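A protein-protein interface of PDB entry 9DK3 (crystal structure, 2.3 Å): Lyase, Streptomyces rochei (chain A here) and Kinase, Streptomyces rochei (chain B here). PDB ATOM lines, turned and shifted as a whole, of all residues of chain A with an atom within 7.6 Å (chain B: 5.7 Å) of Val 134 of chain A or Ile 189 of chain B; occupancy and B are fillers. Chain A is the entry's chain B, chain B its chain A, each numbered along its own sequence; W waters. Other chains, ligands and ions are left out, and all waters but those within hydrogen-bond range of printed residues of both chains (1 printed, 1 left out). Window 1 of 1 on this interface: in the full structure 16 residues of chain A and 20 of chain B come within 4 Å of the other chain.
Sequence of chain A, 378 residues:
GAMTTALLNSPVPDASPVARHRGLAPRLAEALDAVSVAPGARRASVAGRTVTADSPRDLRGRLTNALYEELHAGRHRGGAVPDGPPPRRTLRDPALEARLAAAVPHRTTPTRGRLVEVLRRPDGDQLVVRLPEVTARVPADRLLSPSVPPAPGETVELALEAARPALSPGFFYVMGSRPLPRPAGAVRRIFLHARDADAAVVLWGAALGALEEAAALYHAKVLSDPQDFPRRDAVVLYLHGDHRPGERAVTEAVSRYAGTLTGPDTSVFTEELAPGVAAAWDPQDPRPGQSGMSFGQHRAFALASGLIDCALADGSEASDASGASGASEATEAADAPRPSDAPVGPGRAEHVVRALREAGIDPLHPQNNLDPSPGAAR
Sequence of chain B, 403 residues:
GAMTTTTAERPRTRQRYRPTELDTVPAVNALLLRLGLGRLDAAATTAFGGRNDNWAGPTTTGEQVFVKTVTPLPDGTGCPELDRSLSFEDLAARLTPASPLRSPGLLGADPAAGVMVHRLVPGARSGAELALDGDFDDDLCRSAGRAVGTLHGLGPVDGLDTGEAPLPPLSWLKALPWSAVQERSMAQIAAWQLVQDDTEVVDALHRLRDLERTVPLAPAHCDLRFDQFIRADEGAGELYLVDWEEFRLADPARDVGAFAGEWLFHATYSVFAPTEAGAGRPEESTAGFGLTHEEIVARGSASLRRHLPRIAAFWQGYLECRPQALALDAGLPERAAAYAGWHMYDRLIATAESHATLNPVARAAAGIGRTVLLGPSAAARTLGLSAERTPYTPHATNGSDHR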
ATOM      1  N   GLY A 113      30.341  10.138  -4.398  1.00  0.00           N
ATOM      2  CA  GLY A 113      28.983  10.635  -4.531  1.00  0.00           C
ATOM      3  C   GLY A 113      28.013   9.719  -3.790  1.00  0.00           C
ATOM      4  O   GLY A 113      28.409   8.649  -3.346  1.00  0.00           O
ATOM      5  N   VAL A 129      24.585   7.253  -9.379  1.00  0.00           N
ATOM      6  CA  VAL A 129      25.317   7.987  -8.355  1.00  0.00           C
ATOM      7  C   VAL A 129      25.104   9.489  -8.570  1.00  0.00           C
ATOM      8  O   VAL A 129      25.328  10.003  -9.670  1.00  0.00           O
ATOM      9  CB  VAL A 129      26.813   7.589  -8.380  1.00  0.00           C
ATOM     10  CG1 VAL A 129      27.635   8.340  -7.346  1.00  0.00           C
ATOM     11  CG2 VAL A 129      27.006   6.100  -8.174  1.00  0.00           C
ATOM     12  N   ARG A 130      24.665  10.194  -7.518  1.00  0.00           N
ATOM     13  CA  ARG A 130      24.720  11.646  -7.511  1.00  0.00           C
ATOM     14  C   ARG A 130      26.151  12.106  -7.218  1.00  0.00           C
ATOM     15  O   ARG A 130      26.600  12.130  -6.083  1.00  0.00           O
ATOM     16  CB  ARG A 130      23.692  12.235  -6.554  1.00  0.00           C
ATOM     17  CG  ARG A 130      23.707  13.755  -6.494  1.00  0.00           C
ATOM     18  CD  ARG A 130      22.759  14.245  -5.407  1.00  0.00           C
ATOM     19  NE  ARG A 130      22.416  15.659  -5.521  1.00  0.00           N
ATOM     20  CZ  ARG A 130      21.683  16.168  -6.506  1.00  0.00           C
ATOM     21  NH1 ARG A 130      20.786  15.425  -7.141  1.00  0.00           N
ATOM     22  NH2 ARG A 130      21.850  17.435  -6.833  1.00  0.00           N
ATOM     23  N   LEU A 131      26.872  12.477  -8.278  1.00  0.00           N
ATOM     24  CA  LEU A 131      28.120  13.204  -8.169  1.00  0.00           C
ATOM     25  C   LEU A 131      27.774  14.662  -7.876  1.00  0.00           C
ATOM     26  O   LEU A 131      26.593  15.046  -7.916  1.00  0.00           O
ATOM     27  CB  LEU A 131      28.907  13.038  -9.476  1.00  0.00           C
ATOM     28  CG  LEU A 131      29.186  11.586  -9.870  1.00  0.00           C
ATOM     29  CD1 LEU A 131      29.947  11.513 -11.167  1.00  0.00           C
ATOM     30  CD2 LEU A 131      29.957  10.842  -8.794  1.00  0.00           C
ATOM     31  N   PRO A 132      28.763  15.490  -7.461  1.00  0.00           N
ATOM     32  CA  PRO A 132      28.492  16.900  -7.149  1.00  0.00           C
ATOM     33  C   PRO A 132      27.997  17.693  -8.351  1.00  0.00           C
ATOM     34  O   PRO A 132      27.118  18.525  -8.197  1.00  0.00           O
ATOM     35  CB  PRO A 132      29.807  17.495  -6.628  1.00  0.00           C
ATOM     36  CG  PRO A 132      30.689  16.272  -6.335  1.00  0.00           C
ATOM     37  CD  PRO A 132      30.153  15.104  -7.156  1.00  0.00           C
ATOM     38  N   GLU A 133      28.456  17.324  -9.539  1.00  0.00           N
ATOM     39  CA  GLU A 133      28.106  18.076 -10.766  1.00  0.00           C
ATOM     40  C   GLU A 133      26.939  17.452 -11.549  1.00  0.00           C
ATOM     41  O   GLU A 133      26.399  18.152 -12.402  1.00  0.00           O
ATOM     42  CB  GLU A 133      29.358  18.174 -11.630  1.00  0.00           C
ATOM     43  CG  GLU A 133      30.603  18.532 -10.843  1.00  0.00           C
ATOM     44  CD  GLU A 133      31.319  17.358 -10.197  1.00  0.00           C
ATOM     45  OE1 GLU A 133      30.958  16.205 -10.501  1.00  0.00           O
ATOM     46  OE2 GLU A 133      32.234  17.603  -9.390  1.00  0.00           O
ATOM     47  N   VAL A 134      26.576  16.200 -11.297  1.00  0.00           N
ATOM     48  CA  VAL A 134      25.504  15.536 -12.099  1.00  0.00           C
ATOM     49  C   VAL A 134      25.124  14.170 -11.530  1.00  0.00           C
ATOM     50  O   VAL A 134      25.916  13.614 -10.782  1.00  0.00           O
ATOM     51  CB  VAL A 134      25.930  15.375 -13.571  1.00  0.00           C
ATOM     52  CG1 VAL A 134      26.936  14.252 -13.749  1.00  0.00           C
ATOM     53  CG2 VAL A 134      24.743  15.194 -14.501  1.00  0.00           C
ATOM     54  N   THR A 135      23.925  13.693 -11.862  1.00  0.00           N
ATOM     55  CA  THR A 135      23.540  12.305 -11.510  1.00  0.00           C
ATOM     56  C   THR A 135      23.970  11.478 -12.721  1.00  0.00           C
ATOM     57  O   THR A 135      23.642  11.873 -13.841  1.00  0.00           O
ATOM     58  CB  THR A 135      22.089  12.200 -11.037  1.00  0.00           C
ATOM     59  OG1 THR A 135      21.967  12.992  -9.859  1.00  0.00           O
ATOM     60  CG2 THR A 135      21.673  10.779 -10.736  1.00  0.00           C
ATOM     61  N   ALA A 136      24.671  10.382 -12.500  1.00  0.00           N
ATOM     62  CA  ALA A 136      25.298   9.606 -13.552  1.00  0.00           C
ATOM     63  C   ALA A 136      25.083   8.110 -13.298  1.00  0.00           C
ATOM     64  O   ALA A 136      24.821   7.667 -12.177  1.00  0.00           O
ATOM     65  CB  ALA A 136      26.764   9.972 -13.656  1.00  0.00           C
ATOM     66  N   ARG A 137      25.144   7.350 -14.389  1.00  0.00           N
ATOM     67  CA  ARG A 137      24.930   5.912 -14.398  1.00  0.00           C
ATOM     68  C   ARG A 137      26.304   5.311 -14.656  1.00  0.00           C
ATOM     69  O   ARG A 137      26.819   5.488 -15.765  1.00  0.00           O
ATOM     70  CB  ARG A 137      23.906   5.543 -15.476  1.00  0.00           C
ATOM     71  CG  ARG A 137      23.598   4.061 -15.619  1.00  0.00           C
ATOM     72  CD  ARG A 137      22.447   3.772 -16.580  1.00  0.00           C
ATOM     73  NE  ARG A 137      22.923   3.453 -17.924  1.00  0.00           N
ATOM     74  CZ  ARG A 137      22.497   4.035 -19.041  1.00  0.00           C
ATOM     75  NH1 ARG A 137      23.081   3.762 -20.195  1.00  0.00           N
ATOM     76  NH2 ARG A 137      21.500   4.904 -18.997  1.00  0.00           N
ATOM     77  N   ARG A 164      39.556  14.306 -19.369  1.00  0.00           N
ATOM     78  CA  ARG A 164      38.229  14.796 -19.686  1.00  0.00           C
ATOM     79  C   ARG A 164      38.381  15.776 -20.829  1.00  0.00           C
ATOM     80  O   ARG A 164      38.371  16.984 -20.611  1.00  0.00           O
ATOM     81  CB  ARG A 164      37.579  15.572 -18.537  1.00  0.00           C
ATOM     82  CG  ARG A 164      37.391  14.791 -17.251  1.00  0.00           C
ATOM     83  CD  ARG A 164      36.390  13.675 -17.419  1.00  0.00           C
ATOM     84  NE  ARG A 164      36.409  12.860 -16.209  1.00  0.00           N
ATOM     85  CZ  ARG A 164      35.833  13.187 -15.051  1.00  0.00           C
ATOM     86  NH1 ARG A 164      34.892  14.116 -14.987  1.00  0.00           N
ATOM     87  NH2 ARG A 164      36.174  12.536 -13.954  1.00  0.00           N
ATOM     88  N   ALA A 166      36.487  16.789 -23.298  1.00  0.00           N
ATOM     89  CA  ALA A 166      35.357  17.604 -23.732  1.00  0.00           C
ATOM     90  C   ALA A 166      34.934  18.627 -22.682  1.00  0.00           C
ATOM     91  O   ALA A 166      34.147  19.535 -22.973  1.00  0.00           O
ATOM     92  CB  ALA A 166      34.195  16.700 -24.071  1.00  0.00           C
ATOM     93  N   LEU A 167      35.458  18.510 -21.458  1.00  0.00           N
ATOM     94  CA  LEU A 167      34.932  19.306 -20.358  1.00  0.00           C
ATOM     95  C   LEU A 167      35.133  20.810 -20.583  1.00  0.00           C
ATOM     96  O   LEU A 167      34.286  21.632 -20.199  1.00  0.00           O
ATOM     97  CB  LEU A 167      35.585  18.852 -19.052  1.00  0.00           C
ATOM     98  CG  LEU A 167      34.997  19.468 -17.785  1.00  0.00           C
ATOM     99  CD1 LEU A 167      33.514  19.096 -17.632  1.00  0.00           C
ATOM    100  CD2 LEU A 167      35.771  19.010 -16.555  1.00  0.00           C
ATOM    101  N   LEU B 176      22.621  10.428 -16.303  1.00  0.00           N
ATOM    102  CA  LEU B 176      23.415  10.432 -17.519  1.00  0.00           C
ATOM    103  C   LEU B 176      24.338   9.228 -17.509  1.00  0.00           C
ATOM    104  O   LEU B 176      25.012   9.032 -16.512  1.00  0.00           O
ATOM    105  CB  LEU B 176      24.307  11.673 -17.587  1.00  0.00           C
ATOM    106  CG  LEU B 176      23.783  12.862 -18.375  1.00  0.00           C
ATOM    107  CD1 LEU B 176      24.916  13.833 -18.644  1.00  0.00           C
ATOM    108  CD2 LEU B 176      23.189  12.405 -19.678  1.00  0.00           C
ATOM    109  N   VAL B 181      28.746  11.657 -20.082  1.00  0.00           N
ATOM    110  CA  VAL B 181      29.387  12.713 -19.304  1.00  0.00           C
ATOM    111  C   VAL B 181      30.803  13.010 -19.818  1.00  0.00           C
ATOM    112  O   VAL B 181      31.259  14.156 -19.750  1.00  0.00           O
ATOM    113  CB  VAL B 181      29.434  12.323 -17.818  1.00  0.00           C
ATOM    114  CG1 VAL B 181      30.147  13.390 -16.978  1.00  0.00           C
ATOM    115  CG2 VAL B 181      28.039  12.047 -17.284  1.00  0.00           C
ATOM    116  N   ARG B 184      30.726  15.556 -22.833  1.00  0.00           N
ATOM    117  CA  ARG B 184      29.962  16.779 -22.692  1.00  0.00           C
ATOM    118  C   ARG B 184      30.822  17.884 -22.082  1.00  0.00           C
ATOM    119  O   ARG B 184      31.793  17.655 -21.365  1.00  0.00           O
ATOM    120  CB  ARG B 184      28.742  16.524 -21.809  1.00  0.00           C
ATOM    121  CG  ARG B 184      27.791  15.468 -22.342  1.00  0.00           C
ATOM    122  CD  ARG B 184      26.897  16.034 -23.403  1.00  0.00           C
ATOM    123  NE  ARG B 184      25.968  15.015 -23.860  1.00  0.00           N
ATOM    124  CZ  ARG B 184      26.250  14.130 -24.806  1.00  0.00           C
ATOM    125  NH1 ARG B 184      27.509  13.843 -25.093  1.00  0.00           N
ATOM    126  NH2 ARG B 184      25.272  13.553 -25.474  1.00  0.00           N
ATOM    127  N   SER B 185      30.359  19.107 -22.311  1.00  0.00           N
ATOM    128  CA  SER B 185      31.022  20.303 -21.764  1.00  0.00           C
ATOM    129  C   SER B 185      30.562  20.526 -20.339  1.00  0.00           C
ATOM    130  O   SER B 185      29.528  19.980 -19.973  1.00  0.00           O
ATOM    131  CB  SER B 185      30.641  21.474 -22.579  1.00  0.00           C
ATOM    132  OG  SER B 185      29.417  22.024 -22.131  1.00  0.00           O
ATOM    133  N   MET B 186      31.299  21.340 -19.600  1.00  0.00           N
ATOM    134  CA  MET B 186      30.945  21.662 -18.203  1.00  0.00           C
ATOM    135  C   MET B 186      29.562  22.306 -18.160  1.00  0.00           C
ATOM    136  O   MET B 186      28.832  22.047 -17.215  1.00  0.00           O
ATOM    137  CB  MET B 186      31.982  22.627 -17.635  1.00  0.00           C
ATOM    138  CG  MET B 186      32.133  22.581 -16.137  1.00  0.00           C
ATOM    139  SD  MET B 186      33.403  23.741 -15.576  1.00  0.00           S
ATOM    140  CE  MET B 186      34.323  23.992 -17.092  1.00  0.00           C
ATOM    141  N   ALA B 187      29.232  23.109 -19.161  1.00  0.00           N
ATOM    142  CA  ALA B 187      27.928  23.795 -19.195  1.00  0.00           C
ATOM    143  C   ALA B 187      26.820  22.816 -19.568  1.00  0.00           C
ATOM    144  O   ALA B 187      25.741  22.924 -19.003  1.00  0.00           O
ATOM    145  CB  ALA B 187      27.984  24.940 -20.156  1.00  0.00           C
ATOM    146  N   GLN B 188      27.090  21.900 -20.492  1.00  0.00           N
ATOM    147  CA  GLN B 188      26.079  20.892 -20.798  1.00  0.00           C
ATOM    148  C   GLN B 188      25.784  20.039 -19.559  1.00  0.00           C
ATOM    149  O   GLN B 188      24.634  19.733 -19.250  1.00  0.00           O
ATOM    150  CB  GLN B 188      26.506  19.978 -21.939  1.00  0.00           C
ATOM    151  CG  GLN B 188      26.735  20.699 -23.243  1.00  0.00           C
ATOM    152  CD  GLN B 188      27.040  19.759 -24.387  1.00  0.00           C
ATOM    153  OE1 GLN B 188      28.059  19.084 -24.401  1.00  0.00           O
ATOM    154  NE2 GLN B 188      26.201  19.783 -25.410  1.00  0.00           N
ATOM    155  N   ILE B 189      26.831  19.670 -18.832  1.00  0.00           N
ATOM    156  CA  ILE B 189      26.658  18.906 -17.612  1.00  0.00           C
ATOM    157  C   ILE B 189      25.847  19.685 -16.588  1.00  0.00           C
ATOM    158  O   ILE B 189      24.956  19.114 -15.948  1.00  0.00           O
ATOM    159  CB  ILE B 189      28.039  18.492 -17.080  1.00  0.00           C
ATOM    160  CG1 ILE B 189      28.692  17.463 -18.020  1.00  0.00           C
ATOM    161  CG2 ILE B 189      27.926  17.994 -15.640  1.00  0.00           C
ATOM    162  CD1 ILE B 189      30.190  17.295 -17.832  1.00  0.00           C
ATOM    163  N   ALA B 190      26.169  20.977 -16.414  1.00  0.00           N
ATOM    164  CA  ALA B 190      25.451  21.847 -15.476  1.00  0.00           C
ATOM    165  C   ALA B 190      23.971  21.993 -15.848  1.00  0.00           C
ATOM    166  O   ALA B 190      23.143  21.987 -14.940  1.00  0.00           O
ATOM    167  CB  ALA B 190      26.124  23.211 -15.368  1.00  0.00           C
ATOM    168  N   ALA B 191      23.675  22.128 -17.157  1.00  0.00           N
ATOM    169  CA  ALA B 191      22.322  22.160 -17.708  1.00  0.00           C
ATOM    170  C   ALA B 191      21.596  20.832 -17.467  1.00  0.00           C
ATOM    171  O   ALA B 191      20.480  20.832 -16.952  1.00  0.00           O
ATOM    172  CB  ALA B 191      22.366  22.484 -19.198  1.00  0.00           C
ATOM    173  N   TRP B 192      22.243  19.689 -17.763  1.00  0.00           N
ATOM    174  CA  TRP B 192      21.667  18.399 -17.382  1.00  0.00           C
ATOM    175  C   TRP B 192      21.294  18.355 -15.897  1.00  0.00           C
ATOM    176  O   TRP B 192      20.176  17.976 -15.524  1.00  0.00           O
ATOM    177  CB  TRP B 192      22.574  17.225 -17.791  1.00  0.00           C
ATOM    178  CG  TRP B 192      22.331  16.840 -19.222  1.00  0.00           C
ATOM    179  CD1 TRP B 192      23.186  16.948 -20.290  1.00  0.00           C
ATOM    180  CD2 TRP B 192      21.077  16.364 -19.748  1.00  0.00           C
ATOM    181  NE1 TRP B 192      22.560  16.529 -21.436  1.00  0.00           N
ATOM    182  CE2 TRP B 192      21.274  16.146 -21.133  1.00  0.00           C
ATOM    183  CE3 TRP B 192      19.850  16.008 -19.166  1.00  0.00           C
ATOM    184  CZ2 TRP B 192      20.254  15.638 -21.944  1.00  0.00           C
ATOM    185  CZ3 TRP B 192      18.848  15.495 -19.965  1.00  0.00           C
ATOM    186  CH2 TRP B 192      19.046  15.330 -21.341  1.00  0.00           C
ATOM    187  N   GLN B 193      22.207  18.807 -15.042  1.00  0.00           N
ATOM    188  CA  GLN B 193      21.966  18.744 -13.608  1.00  0.00           C
ATOM    189  C   GLN B 193      20.754  19.573 -13.177  1.00  0.00           C
ATOM    190  O   GLN B 193      19.974  19.121 -12.330  1.00  0.00           O
ATOM    191  CB  GLN B 193      23.217  19.166 -12.848  1.00  0.00           C
ATOM    192  CG  GLN B 193      22.959  19.190 -11.356  1.00  0.00           C
ATOM    193  CD  GLN B 193      24.144  19.755 -10.631  1.00  0.00           C
ATOM    194  OE1 GLN B 193      24.598  20.871 -10.911  1.00  0.00           O
ATOM    195  NE2 GLN B 193      24.631  18.953  -9.694  1.00  0.00           N
ATOM    196  N   LEU B 194      20.607  20.778 -13.741  1.00  0.00           N
ATOM    197  CA  LEU B 194      19.453  21.620 -13.455  1.00  0.00           C
ATOM    198  C   LEU B 194      18.178  20.888 -13.845  1.00  0.00           C
ATOM    199  O   LEU B 194      17.184  20.966 -13.129  1.00  0.00           O
ATOM    200  CB  LEU B 194      19.515  22.920 -14.276  1.00  0.00           C
ATOM    201  CG  LEU B 194      20.664  23.886 -13.989  1.00  0.00           C
ATOM    202  CD1 LEU B 194      20.473  25.163 -14.795  1.00  0.00           C
ATOM    203  CD2 LEU B 194      20.796  24.193 -12.507  1.00  0.00           C
ATOM    204  N   GLN B 196      17.839  17.577 -14.134  1.00  0.00           N
ATOM    205  CA  GLN B 196      17.679  16.351 -13.369  1.00  0.00           C
ATOM    206  C   GLN B 196      17.075  16.666 -11.997  1.00  0.00           C
ATOM    207  O   GLN B 196      16.340  15.843 -11.459  1.00  0.00           O
ATOM    208  CB  GLN B 196      19.007  15.604 -13.185  1.00  0.00           C
ATOM    209  CG  GLN B 196      19.594  14.991 -14.451  1.00  0.00           C
ATOM    210  CD  GLN B 196      20.917  14.304 -14.185  1.00  0.00           C
ATOM    211  OE1 GLN B 196      21.684  14.733 -13.330  1.00  0.00           O
ATOM    212  NE2 GLN B 196      21.206  13.240 -14.924  1.00  0.00           N
HETATM  213  O   HOH W   1      21.558  15.525 -10.583  1.00  0.00           O
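N of Leu 176 of chain B sits close to NE2 of Gln 196 of chain B (3.4 Å).
The side-chain hydroxyl of Ser 185 of chain B lies close to the backbone NH of Ala 187 of chain B (3.2 Å).
The backbone NH (N) of Gln 188 of chain B lies within hydrogen-bond range of the side-chain hydroxyl (OG) of Ser 185 of chain B, at 2.8 Å.
The backbone NH (N) of Val 129 of chain A is in hydrogen-bond range of the backbone carbonyl oxygen (O) of Ala 136 of chain A, 2.8 Å away.
O of Thr 135 of chain A lies within hydrogen-bond range of N of Leu 176 of chain B.
The backbone carbonyl oxygen (O) of Leu 176 of chain B sits at hydrogen-bond distance from the backbone NH (N) of Arg 137 of chain A (2.7 Å).
N of Met 186 of chain B sits at hydrogen-bond distance from O of Leu 167 of chain A (3.1 Å).
NE2 of Gln 193 of chain B lies within hydrogen-bond range of O of Pro 132 of chain A (2.9 Å).
The side-chain amide nitrogen (NE2) of Gln 193 of chain B sits close to the backbone carbonyl oxygen (O) of Glu 133 of chain A.
The side-chain amide oxygen of Gln 196 of chain B is in hydrogen-bond range of the backbone NH of Thr 135 of chain A.
The backbone carbonyl oxygen (O) of Ala 166 of chain A lies close to the backbone carbonyl oxygen (O) of Arg 184 of chain B (3.4 Å).
Of the 13 printed residues of chain A, 8 touch a printed residue of chain B.
Printed residues of chain A that touch a printed residue of chain B: Pro 132, Glu 133, Val 134, Thr 135, Ala 136, Arg 137, Ala 166 and Leu 167.
Hydrophobic or aromatic side chains of chain A that line the printed part of chain B: Val 134, Ala 136, Ala 166 and Leu 167.
Printed residues of chain B that touch a printed residue of chain A: Leu 176, Arg 184, Ser 185, Met 186, Ile 189, Gln 193 and Gln 196.
Of chain B, only Ile 189, Gln 193 and Gln 196 come within 4 Å of Val 134 of chain A.
Of chain A, only Glu 133 (3.6 Å), Val 134 (3.9 Å) and Leu 167 (3.8 Å) come within 4 Å of Ile 189 of chain B.
Printed residues of chain A within 4 Å of Gln 193 of chain B: Pro 132, Glu 133 and Val 134.
Of the printed residues of chain A, Met 186 of chain B touches Leu 167 (3.1 Å).
Of the printed residues of chain A, Arg 184 of chain B touches Ala 166 (3.4 Å) and Leu 167 (3.7 Å).
Of the printed residues of chain A, Ser 185 of chain B touches Ala 166 (3.4 Å) and Leu 167 (3.9 Å).
The nearest residue of chain B that does not touch Val 134 of chain A is Val 181 of chain B (4.3 Å).
The nearest residue of chain A that does not touch Ile 189 of chain B is Arg 164 of chain A (6.3 Å).
The nearest printed residue of chain A that does not touch Leu 176 of chain B is Val 134 of chain A (4.4 Å).
Water W1 bridges OG1 of Thr 135 of chain A and OE1 of Gln 196 of chain B.
Among the printed residues, pairs that only touch across the chains: Glu 133 of chain A with Ile 189 of chain B, Val 134 of chain A with Ile 189 of chain B, Val 134 of chain A with Gln 193 of chain B, Val 134 of chain A with Gln 196 of chain B, Ala 136 of chain A with Leu 176 of chain B, Ala 166 of chain A with Ser 185 of chain B, Leu 167 of chain A with Arg 184 of chain B, Leu 167 of chain A with Ser 185 of chain B and Leu 167 of chain A with Ile 189 of chain B.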
